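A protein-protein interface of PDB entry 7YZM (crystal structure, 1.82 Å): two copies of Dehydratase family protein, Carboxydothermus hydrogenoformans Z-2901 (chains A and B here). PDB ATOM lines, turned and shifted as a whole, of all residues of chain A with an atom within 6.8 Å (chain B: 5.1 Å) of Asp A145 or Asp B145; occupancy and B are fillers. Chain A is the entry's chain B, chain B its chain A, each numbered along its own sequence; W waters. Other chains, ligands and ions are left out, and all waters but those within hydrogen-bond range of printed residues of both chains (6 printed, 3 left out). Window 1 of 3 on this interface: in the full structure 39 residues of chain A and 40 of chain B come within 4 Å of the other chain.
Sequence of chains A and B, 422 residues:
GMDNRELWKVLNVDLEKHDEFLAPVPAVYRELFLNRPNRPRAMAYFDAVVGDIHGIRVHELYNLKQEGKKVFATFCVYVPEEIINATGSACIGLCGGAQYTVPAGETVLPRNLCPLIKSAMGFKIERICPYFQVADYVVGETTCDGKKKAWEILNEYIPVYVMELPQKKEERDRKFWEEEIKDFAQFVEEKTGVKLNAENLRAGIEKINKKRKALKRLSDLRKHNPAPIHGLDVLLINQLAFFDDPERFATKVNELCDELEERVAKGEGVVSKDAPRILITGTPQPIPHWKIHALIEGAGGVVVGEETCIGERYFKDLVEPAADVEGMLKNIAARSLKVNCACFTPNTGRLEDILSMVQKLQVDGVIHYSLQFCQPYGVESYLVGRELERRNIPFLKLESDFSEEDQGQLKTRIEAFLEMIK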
ATOM      1  N   LEU A 113      -1.585 -10.371 -32.751  1.00  0.00           N
ATOM      2  CA  LEU A 113      -2.676 -11.052 -32.086  1.00  0.00           C
ATOM      3  C   LEU A 113      -3.591 -11.596 -33.169  1.00  0.00           C
ATOM      4  O   LEU A 113      -3.593 -11.106 -34.300  1.00  0.00           O
ATOM      5  CB  LEU A 113      -3.437 -10.112 -31.142  1.00  0.00           C
ATOM      6  CG  LEU A 113      -4.171 -10.825 -30.007  1.00  0.00           C
ATOM      7  CD1 LEU A 113      -3.194 -11.367 -28.968  1.00  0.00           C
ATOM      8  CD2 LEU A 113      -5.187  -9.921 -29.341  1.00  0.00           C
ATOM      9  N   ILE A 117      -9.810 -11.555 -33.010  1.00  0.00           N
ATOM     10  CA  ILE A 117      -9.933 -10.707 -31.830  1.00  0.00           C
ATOM     11  C   ILE A 117      -9.775  -9.238 -32.207  1.00  0.00           C
ATOM     12  O   ILE A 117     -10.573  -8.389 -31.794  1.00  0.00           O
ATOM     13  CB  ILE A 117      -8.905 -11.124 -30.763  1.00  0.00           C
ATOM     14  CG1 ILE A 117      -9.038 -12.621 -30.463  1.00  0.00           C
ATOM     15  CG2 ILE A 117      -9.081 -10.287 -29.503  1.00  0.00           C
ATOM     16  CD1 ILE A 117      -7.910 -13.171 -29.639  1.00  0.00           C
ATOM     17  N   THR A 142     -12.810 -17.854 -20.835  1.00  0.00           N
ATOM     18  CA  THR A 142     -11.361 -17.979 -20.647  1.00  0.00           C
ATOM     19  C   THR A 142     -10.858 -19.131 -21.514  1.00  0.00           C
ATOM     20  O   THR A 142     -10.575 -20.235 -21.041  1.00  0.00           O
ATOM     21  CB  THR A 142     -11.015 -18.185 -19.175  1.00  0.00           C
ATOM     22  OG1 THR A 142     -11.624 -19.388 -18.681  1.00  0.00           O
ATOM     23  CG2 THR A 142     -11.489 -17.004 -18.332  1.00  0.00           C
ATOM     24  N   THR A 143     -10.769 -18.864 -22.821  1.00  0.00           N
ATOM     25  CA  THR A 143     -10.249 -19.832 -23.783  1.00  0.00           C
ATOM     26  C   THR A 143      -8.796 -19.498 -24.108  1.00  0.00           C
ATOM     27  O   THR A 143      -7.893 -19.852 -23.344  1.00  0.00           O
ATOM     28  CB  THR A 143     -11.105 -19.846 -25.054  1.00  0.00           C
ATOM     29  OG1 THR A 143     -11.372 -18.503 -25.468  1.00  0.00           O
ATOM     30  CG2 THR A 143     -12.408 -20.581 -24.801  1.00  0.00           C
ATOM     31  N   CYS A 144      -8.557 -18.792 -25.209  1.00  0.00           N
ATOM     32  CA  CYS A 144      -7.191 -18.450 -25.572  1.00  0.00           C
ATOM     33  C   CYS A 144      -6.729 -17.200 -24.817  1.00  0.00           C
ATOM     34  O   CYS A 144      -7.524 -16.426 -24.281  1.00  0.00           O
ATOM     35  CB  CYS A 144      -7.076 -18.225 -27.078  1.00  0.00           C
ATOM     36  SG  CYS A 144      -8.094 -16.854 -27.655  1.00  0.00           S
ATOM     37  N   ASP A 145      -5.412 -17.008 -24.794  1.00  0.00           N
ATOM     38  CA  ASP A 145      -4.839 -15.880 -24.062  1.00  0.00           C
ATOM     39  C   ASP A 145      -5.366 -14.549 -24.581  1.00  0.00           C
ATOM     40  O   ASP A 145      -5.681 -13.644 -23.795  1.00  0.00           O
ATOM     41  CB  ASP A 145      -3.320 -15.902 -24.181  1.00  0.00           C
ATOM     42  CG  ASP A 145      -2.692 -17.093 -23.504  1.00  0.00           C
ATOM     43  OD1 ASP A 145      -3.284 -17.649 -22.551  1.00  0.00           O
ATOM     44  OD2 ASP A 145      -1.581 -17.458 -23.928  1.00  0.00           O
ATOM     45  N   GLY A 146      -5.428 -14.399 -25.905  1.00  0.00           N
ATOM     46  CA  GLY A 146      -5.816 -13.125 -26.480  1.00  0.00           C
ATOM     47  C   GLY A 146      -7.238 -12.731 -26.133  1.00  0.00           C
ATOM     48  O   GLY A 146      -7.509 -11.571 -25.815  1.00  0.00           O
ATOM     49  N   LYS A 147      -8.168 -13.685 -26.201  1.00  0.00           N
ATOM     50  CA  LYS A 147      -9.545 -13.387 -25.820  1.00  0.00           C
ATOM     51  C   LYS A 147      -9.639 -13.077 -24.334  1.00  0.00           C
ATOM     52  O   LYS A 147     -10.249 -12.079 -23.934  1.00  0.00           O
ATOM     53  CB  LYS A 147     -10.468 -14.560 -26.167  1.00  0.00           C
ATOM     54  CG  LYS A 147     -10.968 -14.594 -27.604  1.00  0.00           C
ATOM     55  CD  LYS A 147     -11.686 -15.924 -27.888  1.00  0.00           C
ATOM     56  CE  LYS A 147     -12.865 -15.759 -28.835  1.00  0.00           C
ATOM     57  NZ  LYS A 147     -13.702 -17.001 -28.867  1.00  0.00           N
ATOM     58  N   LYS A 148      -9.034 -13.924 -23.499  1.00  0.00           N
ATOM     59  CA  LYS A 148      -9.141 -13.755 -22.052  1.00  0.00           C
ATOM     60  C   LYS A 148      -8.674 -12.377 -21.618  1.00  0.00           C
ATOM     61  O   LYS A 148      -9.311 -11.734 -20.774  1.00  0.00           O
ATOM     62  CB  LYS A 148      -8.334 -14.839 -21.327  1.00  0.00           C
ATOM     63  CG  LYS A 148      -8.201 -14.603 -19.820  1.00  0.00           C
ATOM     64  CD  LYS A 148      -7.549 -15.785 -19.115  1.00  0.00           C
ATOM     65  CE  LYS A 148      -6.150 -16.084 -19.645  1.00  0.00           C
ATOM     66  NZ  LYS A 148      -5.556 -17.286 -18.963  1.00  0.00           N
ATOM     67  N   LYS A 149      -7.557 -11.904 -22.169  1.00  0.00           N
ATOM     68  CA  LYS A 149      -7.045 -10.602 -21.763  1.00  0.00           C
ATOM     69  C   LYS A 149      -7.755  -9.463 -22.481  1.00  0.00           C
ATOM     70  O   LYS A 149      -7.857  -8.362 -21.932  1.00  0.00           O
ATOM     71  CB  LYS A 149      -5.541 -10.542 -22.000  1.00  0.00           C
ATOM     72  CG  LYS A 149      -4.758 -11.645 -21.285  1.00  0.00           C
ATOM     73  CD  LYS A 149      -5.079 -11.733 -19.798  1.00  0.00           C
ATOM     74  CE  LYS A 149      -4.338 -10.640 -19.033  1.00  0.00           C
ATOM     75  NZ  LYS A 149      -4.690 -10.601 -17.590  1.00  0.00           N
ATOM     76  N   ALA A 150      -8.262  -9.704 -23.689  1.00  0.00           N
ATOM     77  CA  ALA A 150      -9.015  -8.664 -24.381  1.00  0.00           C
ATOM     78  C   ALA A 150     -10.316  -8.334 -23.659  1.00  0.00           C
ATOM     79  O   ALA A 150     -10.787  -7.190 -23.742  1.00  0.00           O
ATOM     80  CB  ALA A 150      -9.302  -9.090 -25.820  1.00  0.00           C
ATOM     81  N   GLN A 167      -9.402 -26.183 -18.291  1.00  0.00           N
ATOM     82  CA  GLN A 167      -8.442 -26.468 -19.344  1.00  0.00           C
ATOM     83  C   GLN A 167      -8.195 -27.961 -19.505  1.00  0.00           C
ATOM     84  O   GLN A 167      -7.398 -28.355 -20.359  1.00  0.00           O
ATOM     85  CB  GLN A 167      -7.128 -25.722 -19.068  1.00  0.00           C
ATOM     86  CG  GLN A 167      -7.336 -24.195 -19.037  1.00  0.00           C
ATOM     87  CD  GLN A 167      -6.071 -23.406 -18.741  1.00  0.00           C
ATOM     88  OE1 GLN A 167      -5.309 -23.081 -19.643  1.00  0.00           O
ATOM     89  NE2 GLN A 167      -5.869 -23.060 -17.481  1.00  0.00           N
ATOM     90  N   CYS A 343      -8.026 -25.364 -26.857  1.00  0.00           N
ATOM     91  CA  CYS A 343      -7.702 -24.776 -25.562  1.00  0.00           C
ATOM     92  C   CYS A 343      -7.717 -25.807 -24.437  1.00  0.00           C
ATOM     93  O   CYS A 343      -7.291 -25.488 -23.323  1.00  0.00           O
ATOM     94  CB  CYS A 343      -8.667 -23.626 -25.254  1.00  0.00           C
ATOM     95  SG  CYS A 343      -8.436 -22.166 -26.324  1.00  0.00           S
ATOM     96  N   PHE A 373      -1.299 -16.207 -35.680  1.00  0.00           N
ATOM     97  CA  PHE A 373      -1.118 -15.904 -34.265  1.00  0.00           C
ATOM     98  C   PHE A 373      -2.123 -16.616 -33.371  1.00  0.00           C
ATOM     99  O   PHE A 373      -2.176 -16.329 -32.171  1.00  0.00           O
ATOM    100  CB  PHE A 373      -1.158 -14.391 -34.009  1.00  0.00           C
ATOM    101  CG  PHE A 373      -0.183 -13.631 -34.852  1.00  0.00           C
ATOM    102  CD1 PHE A 373       1.176 -13.825 -34.696  1.00  0.00           C
ATOM    103  CD2 PHE A 373      -0.621 -12.745 -35.820  1.00  0.00           C
ATOM    104  CE1 PHE A 373       2.080 -13.142 -35.483  1.00  0.00           C
ATOM    105  CE2 PHE A 373       0.279 -12.058 -36.613  1.00  0.00           C
ATOM    106  CZ  PHE A 373       1.629 -12.262 -36.449  1.00  0.00           C
ATOM    107  N   CYS A 374      -2.913 -17.550 -33.906  1.00  0.00           N
ATOM    108  CA  CYS A 374      -3.711 -18.422 -33.053  1.00  0.00           C
ATOM    109  C   CYS A 374      -2.777 -19.503 -32.517  1.00  0.00           C
ATOM    110  O   CYS A 374      -2.422 -20.444 -33.234  1.00  0.00           O
ATOM    111  CB  CYS A 374      -4.876 -19.052 -33.806  1.00  0.00           C
ATOM    112  SG  CYS A 374      -5.626 -20.341 -32.801  1.00  0.00           S
ATOM    113  N   GLN A 375      -2.413 -19.408 -31.257  1.00  0.00           N
ATOM    114  CA  GLN A 375      -1.397 -20.308 -30.726  1.00  0.00           C
ATOM    115  C   GLN A 375      -1.982 -21.657 -30.310  1.00  0.00           C
ATOM    116  O   GLN A 375      -1.310 -22.679 -30.468  1.00  0.00           O
ATOM    117  CB  GLN A 375      -0.663 -19.613 -29.571  1.00  0.00           C
ATOM    118  CG  GLN A 375       0.188 -18.428 -30.064  1.00  0.00           C
ATOM    119  CD  GLN A 375       0.650 -17.468 -28.968  1.00  0.00           C
ATOM    120  OE1 GLN A 375       0.072 -17.405 -27.883  1.00  0.00           O
ATOM    121  NE2 GLN A 375       1.700 -16.710 -29.263  1.00  0.00           N
ATOM    122  N   PRO A 376      -3.213 -21.730 -29.790  1.00  0.00           N
ATOM    123  CA  PRO A 376      -3.752 -23.067 -29.473  1.00  0.00           C
ATOM    124  C   PRO A 376      -3.801 -23.994 -30.683  1.00  0.00           C
ATOM    125  O   PRO A 376      -3.313 -25.131 -30.613  1.00  0.00           O
ATOM    126  CB  PRO A 376      -5.145 -22.754 -28.909  1.00  0.00           C
ATOM    127  CG  PRO A 376      -4.982 -21.409 -28.285  1.00  0.00           C
ATOM    128  CD  PRO A 376      -4.046 -20.654 -29.209  1.00  0.00           C
ATOM    129  N   VAL A 379      -0.086 -24.459 -32.428  1.00  0.00           N
ATOM    130  CA  VAL A 379       0.784 -25.451 -31.810  1.00  0.00           C
ATOM    131  C   VAL A 379       0.226 -26.852 -32.034  1.00  0.00           C
ATOM    132  O   VAL A 379       0.960 -27.777 -32.400  1.00  0.00           O
ATOM    133  CB  VAL A 379       0.979 -25.155 -30.314  1.00  0.00           C
ATOM    134  CG1 VAL A 379       1.835 -26.241 -29.694  1.00  0.00           C
ATOM    135  CG2 VAL A 379       1.626 -23.789 -30.107  1.00  0.00           C
ATOM    136  N   THR B 143      -0.637 -22.476 -17.943  1.00  0.00           N
ATOM    137  CA  THR B 143      -0.590 -21.022 -17.937  1.00  0.00           C
ATOM    138  C   THR B 143      -0.890 -20.469 -19.326  1.00  0.00           C
ATOM    139  O   THR B 143      -2.057 -20.378 -19.720  1.00  0.00           O
ATOM    140  CB  THR B 143       0.769 -20.529 -17.435  1.00  0.00           C
ATOM    141  OG1 THR B 143       1.818 -21.279 -18.063  1.00  0.00           O
ATOM    142  CG2 THR B 143       0.853 -20.682 -15.921  1.00  0.00           C
ATOM    143  N   CYS B 144       0.140 -20.079 -20.074  1.00  0.00           N
ATOM    144  CA  CYS B 144      -0.095 -19.502 -21.389  1.00  0.00           C
ATOM    145  C   CYS B 144      -0.390 -20.601 -22.407  1.00  0.00           C
ATOM    146  O   CYS B 144      -0.139 -21.787 -22.173  1.00  0.00           O
ATOM    147  CB  CYS B 144       1.104 -18.671 -21.831  1.00  0.00           C
ATOM    148  SG  CYS B 144       2.591 -19.669 -21.969  1.00  0.00           S
ATOM    149  N   ASP B 145      -0.959 -20.184 -23.545  1.00  0.00           N
ATOM    150  CA  ASP B 145      -1.340 -21.126 -24.590  1.00  0.00           C
ATOM    151  C   ASP B 145      -0.133 -21.913 -25.089  1.00  0.00           C
ATOM    152  O   ASP B 145      -0.208 -23.133 -25.284  1.00  0.00           O
ATOM    153  CB  ASP B 145      -1.981 -20.376 -25.763  1.00  0.00           C
ATOM    154  CG  ASP B 145      -3.324 -19.769 -25.421  1.00  0.00           C
ATOM    155  OD1 ASP B 145      -3.947 -20.206 -24.434  1.00  0.00           O
ATOM    156  OD2 ASP B 145      -3.748 -18.841 -26.150  1.00  0.00           O
ATOM    157  N   GLY B 146       0.985 -21.222 -25.305  1.00  0.00           N
ATOM    158  CA  GLY B 146       2.153 -21.866 -25.882  1.00  0.00           C
ATOM    159  C   GLY B 146       2.712 -22.966 -25.001  1.00  0.00           C
ATOM    160  O   GLY B 146       3.010 -24.065 -25.472  1.00  0.00           O
ATOM    161  N   LYS B 147       2.883 -22.679 -23.712  1.00  0.00           N
ATOM    162  CA  LYS B 147       3.375 -23.693 -22.782  1.00  0.00           C
ATOM    163  C   LYS B 147       2.393 -24.848 -22.667  1.00  0.00           C
ATOM    164  O   LYS B 147       2.776 -26.023 -22.720  1.00  0.00           O
ATOM    165  CB  LYS B 147       3.596 -23.083 -21.401  1.00  0.00           C
ATOM    166  CG  LYS B 147       4.903 -22.374 -21.216  1.00  0.00           C
ATOM    167  CD  LYS B 147       4.916 -21.676 -19.874  1.00  0.00           C
ATOM    168  CE  LYS B 147       6.328 -21.404 -19.415  1.00  0.00           C
ATOM    169  NZ  LYS B 147       6.336 -20.666 -18.126  1.00  0.00           N
ATOM    170  N   LYS B 148       1.114 -24.526 -22.481  1.00  0.00           N
ATOM    171  CA  LYS B 148       0.104 -25.563 -22.304  1.00  0.00           C
ATOM    172  C   LYS B 148       0.134 -26.563 -23.451  1.00  0.00           C
ATOM    173  O   LYS B 148       0.120 -27.780 -23.237  1.00  0.00           O
ATOM    174  CB  LYS B 148      -1.283 -24.926 -22.192  1.00  0.00           C
ATOM    175  CG  LYS B 148      -2.401 -25.939 -22.047  1.00  0.00           C
ATOM    176  CD  LYS B 148      -3.720 -25.282 -21.696  1.00  0.00           C
ATOM    177  CE  LYS B 148      -4.160 -24.308 -22.780  1.00  0.00           C
ATOM    178  NZ  LYS B 148      -5.513 -23.753 -22.480  1.00  0.00           N
ATOM    179  N   LYS B 149       0.147 -26.068 -24.681  1.00  0.00           N
ATOM    180  CA  LYS B 149       0.126 -26.980 -25.813  1.00  0.00           C
ATOM    181  C   LYS B 149       1.504 -27.579 -26.074  1.00  0.00           C
ATOM    182  O   LYS B 149       1.594 -28.687 -26.603  1.00  0.00           O
ATOM    183  CB  LYS B 149      -0.416 -26.254 -27.043  1.00  0.00           C
ATOM    184  CG  LYS B 149      -1.803 -25.642 -26.844  1.00  0.00           C
ATOM    185  CD  LYS B 149      -2.828 -26.656 -26.373  1.00  0.00           C
ATOM    186  CE  LYS B 149      -3.185 -27.630 -27.487  1.00  0.00           C
ATOM    187  NZ  LYS B 149      -4.139 -28.670 -27.013  1.00  0.00           N
ATOM    188  N   ALA B 150       2.578 -26.893 -25.678  1.00  0.00           N
ATOM    189  CA  ALA B 150       3.913 -27.445 -25.882  1.00  0.00           C
ATOM    190  C   ALA B 150       4.170 -28.657 -24.993  1.00  0.00           C
ATOM    191  O   ALA B 150       4.945 -29.544 -25.371  1.00  0.00           O
ATOM    192  CB  ALA B 150       4.977 -26.378 -25.623  1.00  0.00           C
ATOM    193  N   GLN B 375       1.457 -13.289 -25.395  1.00  0.00           N
ATOM    194  CA  GLN B 375       0.185 -12.594 -25.505  1.00  0.00           C
ATOM    195  C   GLN B 375      -0.343 -12.187 -24.132  1.00  0.00           C
ATOM    196  O   GLN B 375      -0.864 -11.073 -23.998  1.00  0.00           O
ATOM    197  CB  GLN B 375      -0.805 -13.465 -26.287  1.00  0.00           C
ATOM    198  CG  GLN B 375      -0.415 -13.518 -27.773  1.00  0.00           C
ATOM    199  CD  GLN B 375      -1.102 -14.610 -28.578  1.00  0.00           C
ATOM    200  OE1 GLN B 375      -1.748 -15.498 -28.030  1.00  0.00           O
ATOM    201  NE2 GLN B 375      -0.955 -14.544 -29.900  1.00  0.00           N
ATOM    202  N   PRO B 376      -0.207 -13.013 -23.085  1.00  0.00           N
ATOM    203  CA  PRO B 376      -0.692 -12.559 -21.763  1.00  0.00           C
ATOM    204  C   PRO B 376      -0.125 -11.209 -21.336  1.00  0.00           C
ATOM    205  O   PRO B 376      -0.892 -10.310 -20.969  1.00  0.00           O
ATOM    206  CB  PRO B 376      -0.270 -13.701 -20.827  1.00  0.00           C
ATOM    207  CG  PRO B 376      -0.345 -14.949 -21.734  1.00  0.00           C
ATOM    208  CD  PRO B 376       0.152 -14.450 -23.085  1.00  0.00           C
HETATM  209  O   HOH W   1      -6.012 -21.759 -24.448  1.00  0.00           O
HETATM  210  O   HOH W   2      -4.450 -20.087 -18.342  1.00  0.00           O
HETATM  211  O   HOH W   3      -3.009 -17.608 -19.998  1.00  0.00           O
HETATM  212  O   HOH W   4      -5.121 -15.598 -28.467  1.00  0.00           O
HETATM  213  O   HOH W   5       0.506 -16.559 -25.592  1.00  0.00           O
HETATM  214  O   HOH W   6      -3.915 -14.464 -30.607  1.00  0.00           O
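Printed residues of chain A that touch a printed residue of chain B: Leu A113, Cys A144, Asp A145, Lys A149, Gln A167, Cys A343, Phe A373, Gln A375, Pro A376 and Val A379. Hydrophobic or aromatic side chains of chain A that line the printed part of chain B: Leu A113, Pro A376 and Val A379. Along chain A the printed residues that touch a printed residue of chain B span positions 113 to 379. Printed residues of chain B that touch a printed residue of chain A: Cys B144, Asp B145, Lys B148, Lys B149, Gln B375 and Pro B376. Hydrophobic or aromatic side chains of chain B within 4 Å of the printed part of chain A: Pro B376. Among the printed residues, no Asp or Glu carboxylate lies within 4 Å of a Lys or Arg side-chain nitrogen of the other chain.
CD1 of Leu A113 touches CG of Gln B375, at 3.7 Å. Cys A144 touches Asp B145 (CB to OD2, 3.5 Å). CA of Cys B144 touches OD2 of Asp A145, at 3.6 Å. OD2 of Asp A145 touches CG of Pro B376, at 3.6 Å. O of Pro B376 touches CE of Lys A149, at 3.97 Å. Pro A376 touches Asp B145. Val A379 touches Lys B149.
Printed residues of chain B within 4 Å of Asp A145: Cys B144 (3.6 Å), Asp B145 (2.8 Å) and Pro B376 (3.6 Å). Of the printed residues of chain B, Gln A375 touches Gln B375. Printed residues of chain B within 4 Å of Gln A167: Lys B148. Printed residues of chain B within 4 Å of Cys A343: Lys B148.
Cys A144 touches Asp B145, and with the chains exchanged Asp A145 touches Cys B144. Asp B145 touches its own counterpart, Asp A145. Lys A149 touches Pro B376, but with the chains exchanged Pro A376 does not touch Lys B149 (4.004 Å). Gln A375 touches its own counterpart, Gln B375. Positions printed for both chains: 143, 144, 145, 146, 147, 148, 149, 150, 375 and 376.
Water W5 lies within hydrogen-bond range of OE1 of Gln A375, OD2 of Asp A145 and N of Gln B375. Water W3 lies within hydrogen-bond range of OD1 of Asp A145 (2.6 Å), NZ of Lys A148 (2.8 Å) and O of Thr B143 (2.9 Å). Water W1 lies within hydrogen-bond range of OD1 of Asp B145 (2.6 Å), NZ of Lys B148 (2.8 Å), O of Thr A143 (2.9 Å) and SG of Cys A343 (3.1 Å). Water W2 lies within hydrogen-bond range of O of Thr B143 (2.8 Å), NZ of Lys A148 (3.1 Å) and OE1 of Gln A167 (3.4 Å). Water W4 lies within hydrogen-bond range of N of Gly A146 and OE1 of Gln B375. Water W6 lies within hydrogen-bond range of the backbone carbonyl oxygen of Phe A373 (3.0 Å) and the side-chain amide nitrogen of Gln B375 (3.0 Å).
N of Asp B145 sits at hydrogen-bond distance from OD2 of Asp A145, 2.8 Å away. O of Cys A343 is in hydrogen-bond range of NZ of Lys B148 (2.6 Å). The side-chain amide nitrogen (NE2) of Gln B375 is in hydrogen-bond range of the backbone carbonyl oxygen (O) of Phe A373. The side-chain amide oxygen of Gln A167 is in hydrogen-bond range of the side-chain amino group of Lys B148 (2.9 Å). The side-chain amide oxygen (OE1) of Gln B375 lies close to the side-chain amide oxygen (OE1) of Gln A375 (2.6 Å).
The side-chain sulfur (SG) of Cys A343 sits at hydrogen-bond distance from the backbone NH (N) of Cys A144. SG of Cys B144 sits close to N of Lys B147 (3.5 Å). N of Lys A147 sits close to SG of Cys A144 (3.5 Å).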
